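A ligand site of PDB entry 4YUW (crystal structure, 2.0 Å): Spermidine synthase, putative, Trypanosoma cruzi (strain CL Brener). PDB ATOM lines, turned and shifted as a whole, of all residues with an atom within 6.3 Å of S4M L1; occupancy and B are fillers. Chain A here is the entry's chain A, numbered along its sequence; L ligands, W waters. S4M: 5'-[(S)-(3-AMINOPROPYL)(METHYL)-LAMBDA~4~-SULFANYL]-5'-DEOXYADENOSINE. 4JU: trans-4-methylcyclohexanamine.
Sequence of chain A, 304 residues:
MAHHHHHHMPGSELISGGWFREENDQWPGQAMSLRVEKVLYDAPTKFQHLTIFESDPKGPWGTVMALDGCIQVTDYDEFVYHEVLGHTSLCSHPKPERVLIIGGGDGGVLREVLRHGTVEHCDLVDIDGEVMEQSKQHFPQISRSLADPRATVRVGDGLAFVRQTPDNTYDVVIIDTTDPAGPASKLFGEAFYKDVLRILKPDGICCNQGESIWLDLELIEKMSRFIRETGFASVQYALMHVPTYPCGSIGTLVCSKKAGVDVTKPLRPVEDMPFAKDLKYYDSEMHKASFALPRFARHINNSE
Met 65 touches S4M L1 (CE to CE, 3.6 Å).
CD1 of Leu 67 touches C3' of S4M L1 (3.5 Å).
Gln 72 touches S4M L1.
Tyr 81 touches S4M L1 (CE2 to CA, 3.6 Å).
CA of Gly 103 touches N3 of S4M L1 (3.5 Å).
Gly 104 touches S4M L1.
Val 125 touches S4M L1.
Asp 128 touches S4M L1.
CG1 of Val 131 touches O3' of S4M L1, 3.6 Å away.
O of Gly 156 touches C2 of S4M L1, 3.7 Å away.
CA of Thr 177 touches O4' of S4M L1, 3.6 Å away.
Leu 187 touches S4M L1 (CD2 to C6, 3.5 Å).
OH of Tyr 245 touches CA of S4M L1, 3.5 Å away.
Hydrophobic or aromatic side chains that line S4M L1: Met 65, Leu 67, Tyr 81, His 82, Ile 127, Val 131, Pro 183, Ala 184 and Leu 187.
Of the 33 residues printed, 24 come within 4 Å of S4M L1.
N of Gly 158 lies within hydrogen-bond range of N1 of S4M L1 (2.8 Å).
A ring nitrogen (NE2) of His 82 is in hydrogen-bond range of a nitrogen (N) of S4M L1, at 2.9 Å.
A nitrogen (N) of S4M L1 lies within salt-bridge range of the side-chain carboxylate (OD2) of Asp 106 (2.5 Å).
O2' of S4M L1 is in hydrogen-bond range of NE2 of Gln 48.
The backbone NH of Thr 178 sits at hydrogen-bond distance from an oxygen (O4') of S4M L1 (3.4 Å).
The side-chain carboxylate (OD2) of Asp 126 is in hydrogen-bond range of an oxygen (O3') of S4M L1, 2.6 Å away.
A nitrogen (N3) of S4M L1 lies within hydrogen-bond range of the backbone NH (N) of Ile 127, at 3.2 Å.
N of S4M L1 is in salt-bridge range of OD2 of Asp 176 (2.8 Å).
The backbone carbonyl oxygen (O) of Pro 183 is in hydrogen-bond range of a nitrogen (N6) of S4M L1 (3.1 Å).
The side-chain carboxylate of Asp 157 is in hydrogen-bond range of a nitrogen (N6) of S4M L1 (2.9 Å).
A nitrogen (N7) of S4M L1 lies within hydrogen-bond range of the backbone NH (N) of Ala 184.
The side-chain hydroxyl (OH) of Tyr 245 sits at hydrogen-bond distance from the backbone carbonyl oxygen (O) of Gln 72, 2.7 Å away.
The backbone carbonyl oxygen (O) of Gly 156 sits at hydrogen-bond distance from the backbone NH (N) of Ile 127.
The backbone NH (N) of Met 65 lies within hydrogen-bond range of the backbone carbonyl oxygen (O) of Val 73 (2.9 Å).
O of Met 65 sits at hydrogen-bond distance from N of Gln 72 (2.7 Å).
N of Gly 156 sits at hydrogen-bond distance from O of Asp 126 (2.9 Å).
The backbone carbonyl oxygen (O) of Asp 176 sits at hydrogen-bond distance from the backbone NH (N) of Gly 104.
N of Gly 103 is in hydrogen-bond range of O of Val 125 (2.8 Å).
The side-chain carboxylate (OD1) of Asp 128 lies within hydrogen-bond range of the backbone NH (N) of Val 131, 3.5 Å away.
Water W1 lies within hydrogen-bond range of OD2 of Asp 176 (2.7 Å), N of Val 109 (2.8 Å), OD1 of Asp 106 (2.9 Å), N of Gly 108 (3.2 Å) and N of S4M L1 (3.3 Å).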
ATOM      1  N   GLN A  48      -0.600 -33.796  23.793  1.00  0.00           N
ATOM      2  CA  GLN A  48       0.633 -34.308  24.323  1.00  0.00           C
ATOM      3  C   GLN A  48       0.553 -34.513  25.838  1.00  0.00           C
ATOM      4  O   GLN A  48      -0.387 -34.039  26.480  1.00  0.00           O
ATOM      5  CB  GLN A  48       1.841 -33.462  23.810  1.00  0.00           C
ATOM      6  CG  GLN A  48       2.018 -32.086  24.271  1.00  0.00           C
ATOM      7  CD  GLN A  48       2.579 -31.081  23.170  1.00  0.00           C
ATOM      8  OE1 GLN A  48       3.606 -31.297  22.456  1.00  0.00           O
ATOM      9  NE2 GLN A  48       1.940 -29.961  23.114  1.00  0.00           N
ATOM     10  N   MET A  65       8.959 -28.016  33.479  1.00  0.00           N
ATOM     11  CA  MET A  65       7.853 -28.449  32.573  1.00  0.00           C
ATOM     12  C   MET A  65       8.418 -29.448  31.562  1.00  0.00           C
ATOM     13  O   MET A  65       9.530 -29.228  31.023  1.00  0.00           O
ATOM     14  CB  MET A  65       7.231 -27.255  31.827  1.00  0.00           C
ATOM     15  CG  MET A  65       6.178 -27.693  30.775  1.00  0.00           C
ATOM     16  SD  MET A  65       5.314 -26.209  30.188  1.00  0.00           S
ATOM     17  CE  MET A  65       6.194 -26.169  28.656  1.00  0.00           C
ATOM     18  N   LEU A  67       7.024 -32.056  28.211  1.00  0.00           N
ATOM     19  CA  LEU A  67       5.968 -32.382  27.210  1.00  0.00           C
ATOM     20  C   LEU A  67       6.394 -33.684  26.575  1.00  0.00           C
ATOM     21  O   LEU A  67       7.509 -33.779  26.046  1.00  0.00           O
ATOM     22  CB  LEU A  67       5.858 -31.269  26.127  1.00  0.00           C
ATOM     23  CG  LEU A  67       4.999 -30.032  26.447  1.00  0.00           C
ATOM     24  CD1 LEU A  67       5.051 -28.915  25.382  1.00  0.00           C
ATOM     25  CD2 LEU A  67       3.557 -30.448  26.754  1.00  0.00           C
ATOM     26  N   GLN A  72      11.043 -28.975  28.809  1.00  0.00           N
ATOM     27  CA  GLN A  72      10.817 -27.788  27.934  1.00  0.00           C
ATOM     28  C   GLN A  72      11.436 -26.548  28.547  1.00  0.00           C
ATOM     29  O   GLN A  72      12.069 -25.717  27.853  1.00  0.00           O
ATOM     30  CB  GLN A  72       9.329 -27.550  27.747  1.00  0.00           C
ATOM     31  CG  GLN A  72       8.628 -28.761  27.083  1.00  0.00           C
ATOM     32  CD  GLN A  72       9.080 -29.012  25.672  1.00  0.00           C
ATOM     33  OE1 GLN A  72       8.924 -28.138  24.796  1.00  0.00           O
ATOM     34  NE2 GLN A  72       9.599 -30.227  25.405  1.00  0.00           N
ATOM     35  N   VAL A  73      11.214 -26.419  29.853  1.00  0.00           N
ATOM     36  CA  VAL A  73      11.636 -25.215  30.588  1.00  0.00           C
ATOM     37  C   VAL A  73      11.941 -25.516  32.065  1.00  0.00           C
ATOM     38  O   VAL A  73      11.264 -26.397  32.655  1.00  0.00           O
ATOM     39  CB  VAL A  73      10.481 -24.200  30.371  1.00  0.00           C
ATOM     40  CG1 VAL A  73       9.876 -23.658  31.634  1.00  0.00           C
ATOM     41  CG2 VAL A  73      10.855 -23.100  29.383  1.00  0.00           C
ATOM     42  N   TYR A  81      17.782 -19.961  26.175  1.00  0.00           N
ATOM     43  CA  TYR A  81      17.186 -20.331  24.859  1.00  0.00           C
ATOM     44  C   TYR A  81      16.249 -19.196  24.408  1.00  0.00           C
ATOM     45  O   TYR A  81      16.172 -18.861  23.216  1.00  0.00           O
ATOM     46  CB  TYR A  81      16.406 -21.629  25.056  1.00  0.00           C
ATOM     47  CG  TYR A  81      15.574 -22.075  23.891  1.00  0.00           C
ATOM     48  CD1 TYR A  81      16.161 -22.735  22.806  1.00  0.00           C
ATOM     49  CD2 TYR A  81      14.193 -21.861  23.877  1.00  0.00           C
ATOM     50  CE1 TYR A  81      15.374 -23.185  21.743  1.00  0.00           C
ATOM     51  CE2 TYR A  81      13.397 -22.302  22.821  1.00  0.00           C
ATOM     52  CZ  TYR A  81      14.006 -22.930  21.760  1.00  0.00           C
ATOM     53  OH  TYR A  81      13.204 -23.387  20.715  1.00  0.00           O
ATOM     54  N   HIS A  82      15.501 -18.615  25.343  1.00  0.00           N
ATOM     55  CA  HIS A  82      14.576 -17.542  24.962  1.00  0.00           C
ATOM     56  C   HIS A  82      15.338 -16.287  24.513  1.00  0.00           C
ATOM     57  O   HIS A  82      14.957 -15.668  23.563  1.00  0.00           O
ATOM     58  CB  HIS A  82      13.655 -17.295  26.144  1.00  0.00           C
ATOM     59  CG  HIS A  82      12.776 -18.475  26.415  1.00  0.00           C
ATOM     60  ND1 HIS A  82      12.433 -18.870  27.697  1.00  0.00           N
ATOM     61  CD2 HIS A  82      12.224 -19.375  25.568  1.00  0.00           C
ATOM     62  CE1 HIS A  82      11.682 -19.962  27.604  1.00  0.00           C
ATOM     63  NE2 HIS A  82      11.571 -20.299  26.320  1.00  0.00           N
ATOM     64  N   ILE A 102       6.066 -19.548  15.991  1.00  0.00           N
ATOM     65  CA  ILE A 102       5.430 -20.838  15.891  1.00  0.00           C
ATOM     66  C   ILE A 102       5.848 -21.660  17.141  1.00  0.00           C
ATOM     67  O   ILE A 102       7.021 -21.807  17.406  1.00  0.00           O
ATOM     68  CB  ILE A 102       5.836 -21.617  14.599  1.00  0.00           C
ATOM     69  CG1 ILE A 102       5.427 -20.889  13.309  1.00  0.00           C
ATOM     70  CG2 ILE A 102       5.201 -23.020  14.600  1.00  0.00           C
ATOM     71  CD1 ILE A 102       3.955 -20.574  13.308  1.00  0.00           C
ATOM     72  N   GLY A 103       4.885 -22.175  17.876  1.00  0.00           N
ATOM     73  CA  GLY A 103       5.198 -22.936  19.108  1.00  0.00           C
ATOM     74  C   GLY A 103       5.255 -21.857  20.161  1.00  0.00           C
ATOM     75  O   GLY A 103       4.466 -20.871  20.091  1.00  0.00           O
ATOM     76  N   GLY A 104       6.190 -21.987  21.086  1.00  0.00           N
ATOM     77  CA  GLY A 104       6.419 -20.899  22.037  1.00  0.00           C
ATOM     78  C   GLY A 104       5.284 -20.608  23.005  1.00  0.00           C
ATOM     79  O   GLY A 104       5.250 -19.500  23.575  1.00  0.00           O
ATOM     80  N   GLY A 105       4.378 -21.583  23.276  1.00  0.00           N
ATOM     81  CA  GLY A 105       3.158 -21.298  24.061  1.00  0.00           C
ATOM     82  C   GLY A 105       3.442 -20.895  25.525  1.00  0.00           C
ATOM     83  O   GLY A 105       2.560 -20.325  26.194  1.00  0.00           O
ATOM     84  N   ASP A 106       4.693 -21.158  25.998  1.00  0.00           N
ATOM     85  CA  ASP A 106       5.147 -20.732  27.339  1.00  0.00           C
ATOM     86  C   ASP A 106       5.346 -19.205  27.462  1.00  0.00           C
ATOM     87  O   ASP A 106       5.350 -18.679  28.592  1.00  0.00           O
ATOM     88  CB  ASP A 106       6.424 -21.456  27.752  1.00  0.00           C
ATOM     89  CG  ASP A 106       7.527 -21.299  26.725  1.00  0.00           C
ATOM     90  OD1 ASP A 106       8.016 -20.178  26.585  1.00  0.00           O
ATOM     91  OD2 ASP A 106       7.876 -22.295  26.015  1.00  0.00           O
ATOM     92  N   GLY A 107       5.523 -18.522  26.329  1.00  0.00           N
ATOM     93  CA  GLY A 107       5.625 -17.036  26.246  1.00  0.00           C
ATOM     94  C   GLY A 107       7.069 -16.506  26.210  1.00  0.00           C
ATOM     95  O   GLY A 107       7.298 -15.270  26.126  1.00  0.00           O
ATOM     96  N   GLY A 108       8.046 -17.421  26.303  1.00  0.00           N
ATOM     97  CA  GLY A 108       9.427 -16.994  26.689  1.00  0.00           C
ATOM     98  C   GLY A 108      10.114 -16.244  25.578  1.00  0.00           C
ATOM     99  O   GLY A 108      10.715 -15.159  25.769  1.00  0.00           O
ATOM    100  N   VAL A 109      10.049 -16.805  24.373  1.00  0.00           N
ATOM    101  CA  VAL A 109      10.590 -16.080  23.204  1.00  0.00           C
ATOM    102  C   VAL A 109       9.804 -14.787  22.999  1.00  0.00           C
ATOM    103  O   VAL A 109      10.377 -13.772  22.639  1.00  0.00           O
ATOM    104  CB  VAL A 109      10.505 -16.927  21.901  1.00  0.00           C
ATOM    105  CG1 VAL A 109      10.858 -16.054  20.710  1.00  0.00           C
ATOM    106  CG2 VAL A 109      11.521 -18.071  21.982  1.00  0.00           C
ATOM    107  N   VAL A 125       1.574 -18.730  17.585  1.00  0.00           N
ATOM    108  CA  VAL A 125       0.664 -19.801  17.282  1.00  0.00           C
ATOM    109  C   VAL A 125       1.208 -21.114  17.853  1.00  0.00           C
ATOM    110  O   VAL A 125       2.190 -21.625  17.320  1.00  0.00           O
ATOM    111  CB  VAL A 125       0.509 -19.971  15.755  1.00  0.00           C
ATOM    112  CG1 VAL A 125      -0.591 -21.010  15.427  1.00  0.00           C
ATOM    113  CG2 VAL A 125       0.131 -18.633  15.120  1.00  0.00           C
ATOM    114  N   ASP A 126       0.500 -21.734  18.798  1.00  0.00           N
ATOM    115  CA  ASP A 126       0.949 -22.981  19.404  1.00  0.00           C
ATOM    116  C   ASP A 126      -0.250 -23.903  19.421  1.00  0.00           C
ATOM    117  O   ASP A 126      -1.382 -23.464  19.703  1.00  0.00           O
ATOM    118  CB  ASP A 126       1.416 -22.716  20.861  1.00  0.00           C
ATOM    119  CG  ASP A 126       2.100 -23.934  21.517  1.00  0.00           C
ATOM    120  OD1 ASP A 126       1.464 -25.022  21.626  1.00  0.00           O
ATOM    121  OD2 ASP A 126       3.273 -23.744  21.983  1.00  0.00           O
ATOM    122  N   ILE A 127       0.020 -25.180  19.123  1.00  0.00           N
ATOM    123  CA  ILE A 127      -1.053 -26.197  18.966  1.00  0.00           C
ATOM    124  C   ILE A 127      -1.737 -26.516  20.304  1.00  0.00           C
ATOM    125  O   ILE A 127      -2.881 -26.946  20.327  1.00  0.00           O
ATOM    126  CB  ILE A 127      -0.478 -27.462  18.274  1.00  0.00           C
ATOM    127  CG1 ILE A 127      -1.607 -28.229  17.486  1.00  0.00           C
ATOM    128  CG2 ILE A 127       0.307 -28.332  19.272  1.00  0.00           C
ATOM    129  CD1 ILE A 127      -1.138 -29.326  16.512  1.00  0.00           C
ATOM    130  N   ASP A 128      -1.052 -26.256  21.436  1.00  0.00           N
ATOM    131  CA  ASP A 128      -1.543 -26.726  22.716  1.00  0.00           C
ATOM    132  C   ASP A 128      -2.002 -25.621  23.730  1.00  0.00           C
ATOM    133  O   ASP A 128      -1.199 -25.050  24.521  1.00  0.00           O
ATOM    134  CB  ASP A 128      -0.461 -27.684  23.321  1.00  0.00           C
ATOM    135  CG  ASP A 128      -1.041 -28.673  24.335  1.00  0.00           C
ATOM    136  OD1 ASP A 128      -1.911 -28.239  25.118  1.00  0.00           O
ATOM    137  OD2 ASP A 128      -0.560 -29.851  24.332  1.00  0.00           O
ATOM    138  N   VAL A 131      -0.732 -25.850  27.331  1.00  0.00           N
ATOM    139  CA  VAL A 131       0.593 -25.364  27.633  1.00  0.00           C
ATOM    140  C   VAL A 131       0.488 -23.899  28.016  1.00  0.00           C
ATOM    141  O   VAL A 131       0.999 -23.468  29.076  1.00  0.00           O
ATOM    142  CB  VAL A 131       1.602 -25.577  26.464  1.00  0.00           C
ATOM    143  CG1 VAL A 131       2.901 -24.835  26.748  1.00  0.00           C
ATOM    144  CG2 VAL A 131       1.886 -27.046  26.254  1.00  0.00           C
ATOM    145  N   GLY A 156      -3.373 -23.220  17.553  1.00  0.00           N
ATOM    146  CA  GLY A 156      -3.594 -23.913  16.275  1.00  0.00           C
ATOM    147  C   GLY A 156      -2.316 -24.562  15.812  1.00  0.00           C
ATOM    148  O   GLY A 156      -1.263 -24.323  16.407  1.00  0.00           O
ATOM    149  N   ASP A 157      -2.400 -25.361  14.738  1.00  0.00           N
ATOM    150  CA  ASP A 157      -1.226 -26.013  14.200  1.00  0.00           C
ATOM    151  C   ASP A 157      -0.430 -24.957  13.394  1.00  0.00           C
ATOM    152  O   ASP A 157      -0.992 -24.256  12.542  1.00  0.00           O
ATOM    153  CB  ASP A 157      -1.639 -27.237  13.381  1.00  0.00           C
ATOM    154  CG  ASP A 157      -0.556 -27.731  12.460  1.00  0.00           C
ATOM    155  OD1 ASP A 157       0.632 -27.688  12.810  1.00  0.00           O
ATOM    156  OD2 ASP A 157      -0.870 -28.117  11.331  1.00  0.00           O
ATOM    157  N   GLY A 158       0.875 -24.853  13.666  1.00  0.00           N
ATOM    158  CA  GLY A 158       1.771 -23.938  12.928  1.00  0.00           C
ATOM    159  C   GLY A 158       1.832 -24.183  11.435  1.00  0.00           C
ATOM    160  O   GLY A 158       1.956 -23.212  10.644  1.00  0.00           O
ATOM    161  N   LEU A 159       1.739 -25.473  11.026  1.00  0.00           N
ATOM    162  CA  LEU A 159       1.838 -25.852   9.606  1.00  0.00           C
ATOM    163  C   LEU A 159       0.683 -25.221   8.807  1.00  0.00           C
ATOM    164  O   LEU A 159       0.907 -24.586   7.789  1.00  0.00           O
ATOM    165  CB  LEU A 159       1.798 -27.395   9.432  1.00  0.00           C
ATOM    166  CG  LEU A 159       2.149 -28.058   8.046  1.00  0.00           C
ATOM    167  CD1 LEU A 159       3.638 -27.920   7.777  1.00  0.00           C
ATOM    168  CD2 LEU A 159       1.879 -29.553   8.020  1.00  0.00           C
ATOM    169  N   ASP A 176       9.795 -22.190  17.512  1.00  0.00           N
ATOM    170  CA  ASP A 176      10.130 -22.661  18.850  1.00  0.00           C
ATOM    171  C   ASP A 176       9.333 -23.921  19.190  1.00  0.00           C
ATOM    172  O   ASP A 176       8.275 -23.848  19.840  1.00  0.00           O
ATOM    173  CB  ASP A 176       9.848 -21.565  19.911  1.00  0.00           C
ATOM    174  CG  ASP A 176      10.128 -22.051  21.325  1.00  0.00           C
ATOM    175  OD1 ASP A 176      10.767 -23.174  21.511  1.00  0.00           O
ATOM    176  OD2 ASP A 176       9.695 -21.331  22.257  1.00  0.00           O
ATOM    177  N   THR A 177       9.812 -25.062  18.698  1.00  0.00           N
ATOM    178  CA  THR A 177       8.998 -26.281  18.759  1.00  0.00           C
ATOM    179  C   THR A 177       9.557 -27.313  19.748  1.00  0.00           C
ATOM    180  O   THR A 177      10.693 -27.253  20.166  1.00  0.00           O
ATOM    181  CB  THR A 177       8.898 -26.965  17.363  1.00  0.00           C
ATOM    182  OG1 THR A 177      10.212 -27.422  17.003  1.00  0.00           O
ATOM    183  CG2 THR A 177       8.386 -25.993  16.296  1.00  0.00           C
ATOM    184  N   THR A 178       8.708 -28.264  20.113  1.00  0.00           N
ATOM    185  CA  THR A 178       9.143 -29.491  20.721  1.00  0.00           C
ATOM    186  C   THR A 178      10.021 -30.302  19.702  1.00  0.00           C
ATOM    187  O   THR A 178      10.158 -29.915  18.539  1.00  0.00           O
ATOM    188  CB  THR A 178       7.892 -30.306  21.117  1.00  0.00           C
ATOM    189  OG1 THR A 178       6.919 -30.245  20.062  1.00  0.00           O
ATOM    190  CG2 THR A 178       7.250 -29.779  22.371  1.00  0.00           C
ATOM    191  N   GLY A 182       6.060 -36.271  17.868  1.00  0.00           N
ATOM    192  CA  GLY A 182       4.825 -35.690  18.411  1.00  0.00           C
ATOM    193  C   GLY A 182       4.270 -34.643  17.448  1.00  0.00           C
ATOM    194  O   GLY A 182       4.560 -34.713  16.261  1.00  0.00           O
ATOM    195  N   PRO A 183       3.451 -33.702  17.948  1.00  0.00           N
ATOM    196  CA  PRO A 183       2.804 -32.809  16.961  1.00  0.00           C
ATOM    197  C   PRO A 183       3.752 -31.858  16.158  1.00  0.00           C
ATOM    198  O   PRO A 183       3.265 -31.267  15.172  1.00  0.00           O
ATOM    199  CB  PRO A 183       1.815 -31.982  17.812  1.00  0.00           C
ATOM    200  CG  PRO A 183       2.437 -32.025  19.180  1.00  0.00           C
ATOM    201  CD  PRO A 183       3.011 -33.401  19.327  1.00  0.00           C
ATOM    202  N   ALA A 184       5.040 -31.724  16.521  1.00  0.00           N
ATOM    203  CA  ALA A 184       5.960 -30.806  15.765  1.00  0.00           C
ATOM    204  C   ALA A 184       6.514 -31.500  14.529  1.00  0.00           C
ATOM    205  O   ALA A 184       7.306 -30.941  13.724  1.00  0.00           O
ATOM    206  CB  ALA A 184       7.111 -30.321  16.645  1.00  0.00           C
ATOM    207  N   SER A 185       6.131 -32.762  14.372  1.00  0.00           N
ATOM    208  CA  SER A 185       6.751 -33.599  13.351  1.00  0.00           C
ATOM    209  C   SER A 185       7.012 -32.882  11.997  1.00  0.00           C
ATOM    210  O   SER A 185       8.176 -32.812  11.539  1.00  0.00           O
ATOM    211  CB  SER A 185       5.895 -34.854  13.077  1.00  0.00           C
ATOM    212  OG  SER A 185       6.671 -35.598  12.187  1.00  0.00           O
ATOM    213  N   LEU A 187       6.865 -29.813  11.138  1.00  0.00           N
ATOM    214  CA  LEU A 187       7.635 -28.584  11.276  1.00  0.00           C
ATOM    215  C   LEU A 187       9.155 -28.752  11.125  1.00  0.00           C
ATOM    216  O   LEU A 187       9.890 -27.788  11.051  1.00  0.00           O
ATOM    217  CB  LEU A 187       7.312 -27.961  12.659  1.00  0.00           C
ATOM    218  CG  LEU A 187       6.028 -27.124  12.918  1.00  0.00           C
ATOM    219  CD1 LEU A 187       4.921 -27.279  11.930  1.00  0.00           C
ATOM    220  CD2 LEU A 187       5.570 -27.041  14.381  1.00  0.00           C
ATOM    221  N   TYR A 245      18.572 -29.231  28.643  1.00  0.00           N
ATOM    222  CA  TYR A 245      18.241 -29.902  27.381  1.00  0.00           C
ATOM    223  C   TYR A 245      19.282 -30.991  27.156  1.00  0.00           C
ATOM    224  O   TYR A 245      20.377 -30.944  27.741  1.00  0.00           O
ATOM    225  CB  TYR A 245      18.203 -28.921  26.223  1.00  0.00           C
ATOM    226  CG  TYR A 245      17.068 -27.924  26.224  1.00  0.00           C
ATOM    227  CD1 TYR A 245      15.789 -28.235  26.784  1.00  0.00           C
ATOM    228  CD2 TYR A 245      17.236 -26.677  25.592  1.00  0.00           C
ATOM    229  CE1 TYR A 245      14.735 -27.281  26.774  1.00  0.00           C
ATOM    230  CE2 TYR A 245      16.183 -25.750  25.562  1.00  0.00           C
ATOM    231  CZ  TYR A 245      14.956 -26.058  26.160  1.00  0.00           C
ATOM    232  OH  TYR A 245      13.960 -25.104  26.094  1.00  0.00           O
HETATM  233  CA  S4M L   1      10.967 -23.511  25.133  1.00  0.00           C
HETATM  234  N   S4M L   1      10.118 -22.318  24.810  1.00  0.00           N
HETATM  235  CB  S4M L   1       9.989 -24.617  25.388  1.00  0.00           C
HETATM  236  CG  S4M L   1       9.543 -25.007  23.990  1.00  0.00           C
HETATM  237  SD  S4M L   1       7.788 -24.539  23.697  1.00  0.00           S
HETATM  238  CE  S4M L   1       7.241 -25.221  25.298  1.00  0.00           C
HETATM  239  C5' S4M L   1       7.394 -25.852  22.448  1.00  0.00           C
HETATM  240  C4' S4M L   1       5.965 -25.781  21.893  1.00  0.00           C
HETATM  241  O4' S4M L   1       5.883 -26.410  20.554  1.00  0.00           O
HETATM  242  C1' S4M L   1       4.445 -26.520  20.435  1.00  0.00           C
HETATM  243  C2' S4M L   1       4.147 -27.322  21.693  1.00  0.00           C
HETATM  244  O2' S4M L   1       2.766 -27.310  22.031  1.00  0.00           O
HETATM  245  C3' S4M L   1       4.999 -26.580  22.738  1.00  0.00           C
HETATM  246  O3' S4M L   1       4.206 -25.686  23.495  1.00  0.00           O
HETATM  247  N9  S4M L   1       4.074 -27.207  19.200  1.00  0.00           N
HETATM  248  C8  S4M L   1       4.344 -28.515  18.874  1.00  0.00           C
HETATM  249  N7  S4M L   1       3.810 -28.812  17.692  1.00  0.00           N
HETATM  250  C5  S4M L   1       3.223 -27.666  17.227  1.00  0.00           C
HETATM  251  C6  S4M L   1       2.544 -27.351  16.058  1.00  0.00           C
HETATM  252  N6  S4M L   1       2.370 -28.306  15.055  1.00  0.00           N
HETATM  253  C4  S4M L   1       3.389 -26.638  18.141  1.00  0.00           C
HETATM  254  N3  S4M L   1       2.973 -25.378  18.003  1.00  0.00           N
HETATM  255  C2  S4M L   1       2.355 -25.209  16.829  1.00  0.00           C
HETATM  256  N1  S4M L   1       2.112 -26.090  15.852  1.00  0.00           N
HETATM  257  N1  4JU L   2      14.708 -31.788  23.589  1.00  0.00           N
HETATM  258  C5  4JU L   2      14.378 -30.338  23.876  1.00  0.00           C
HETATM  259  C6  4JU L   2      14.929 -29.533  22.718  1.00  0.00           C
HETATM  260  C4  4JU L   2      12.843 -30.110  23.971  1.00  0.00           C
HETATM  261  C3  4JU L   2      12.421 -28.622  23.981  1.00  0.00           C
HETATM  262  C2  4JU L   2      13.019 -27.830  22.834  1.00  0.00           C
HETATM  263  C1  4JU L   2      12.797 -26.314  23.042  1.00  0.00           C
HETATM  264  C7  4JU L   2      14.548 -28.020  22.870  1.00  0.00           C
HETATM  265  O   HOH W   1       8.908 -19.356  23.899  1.00  0.00           O
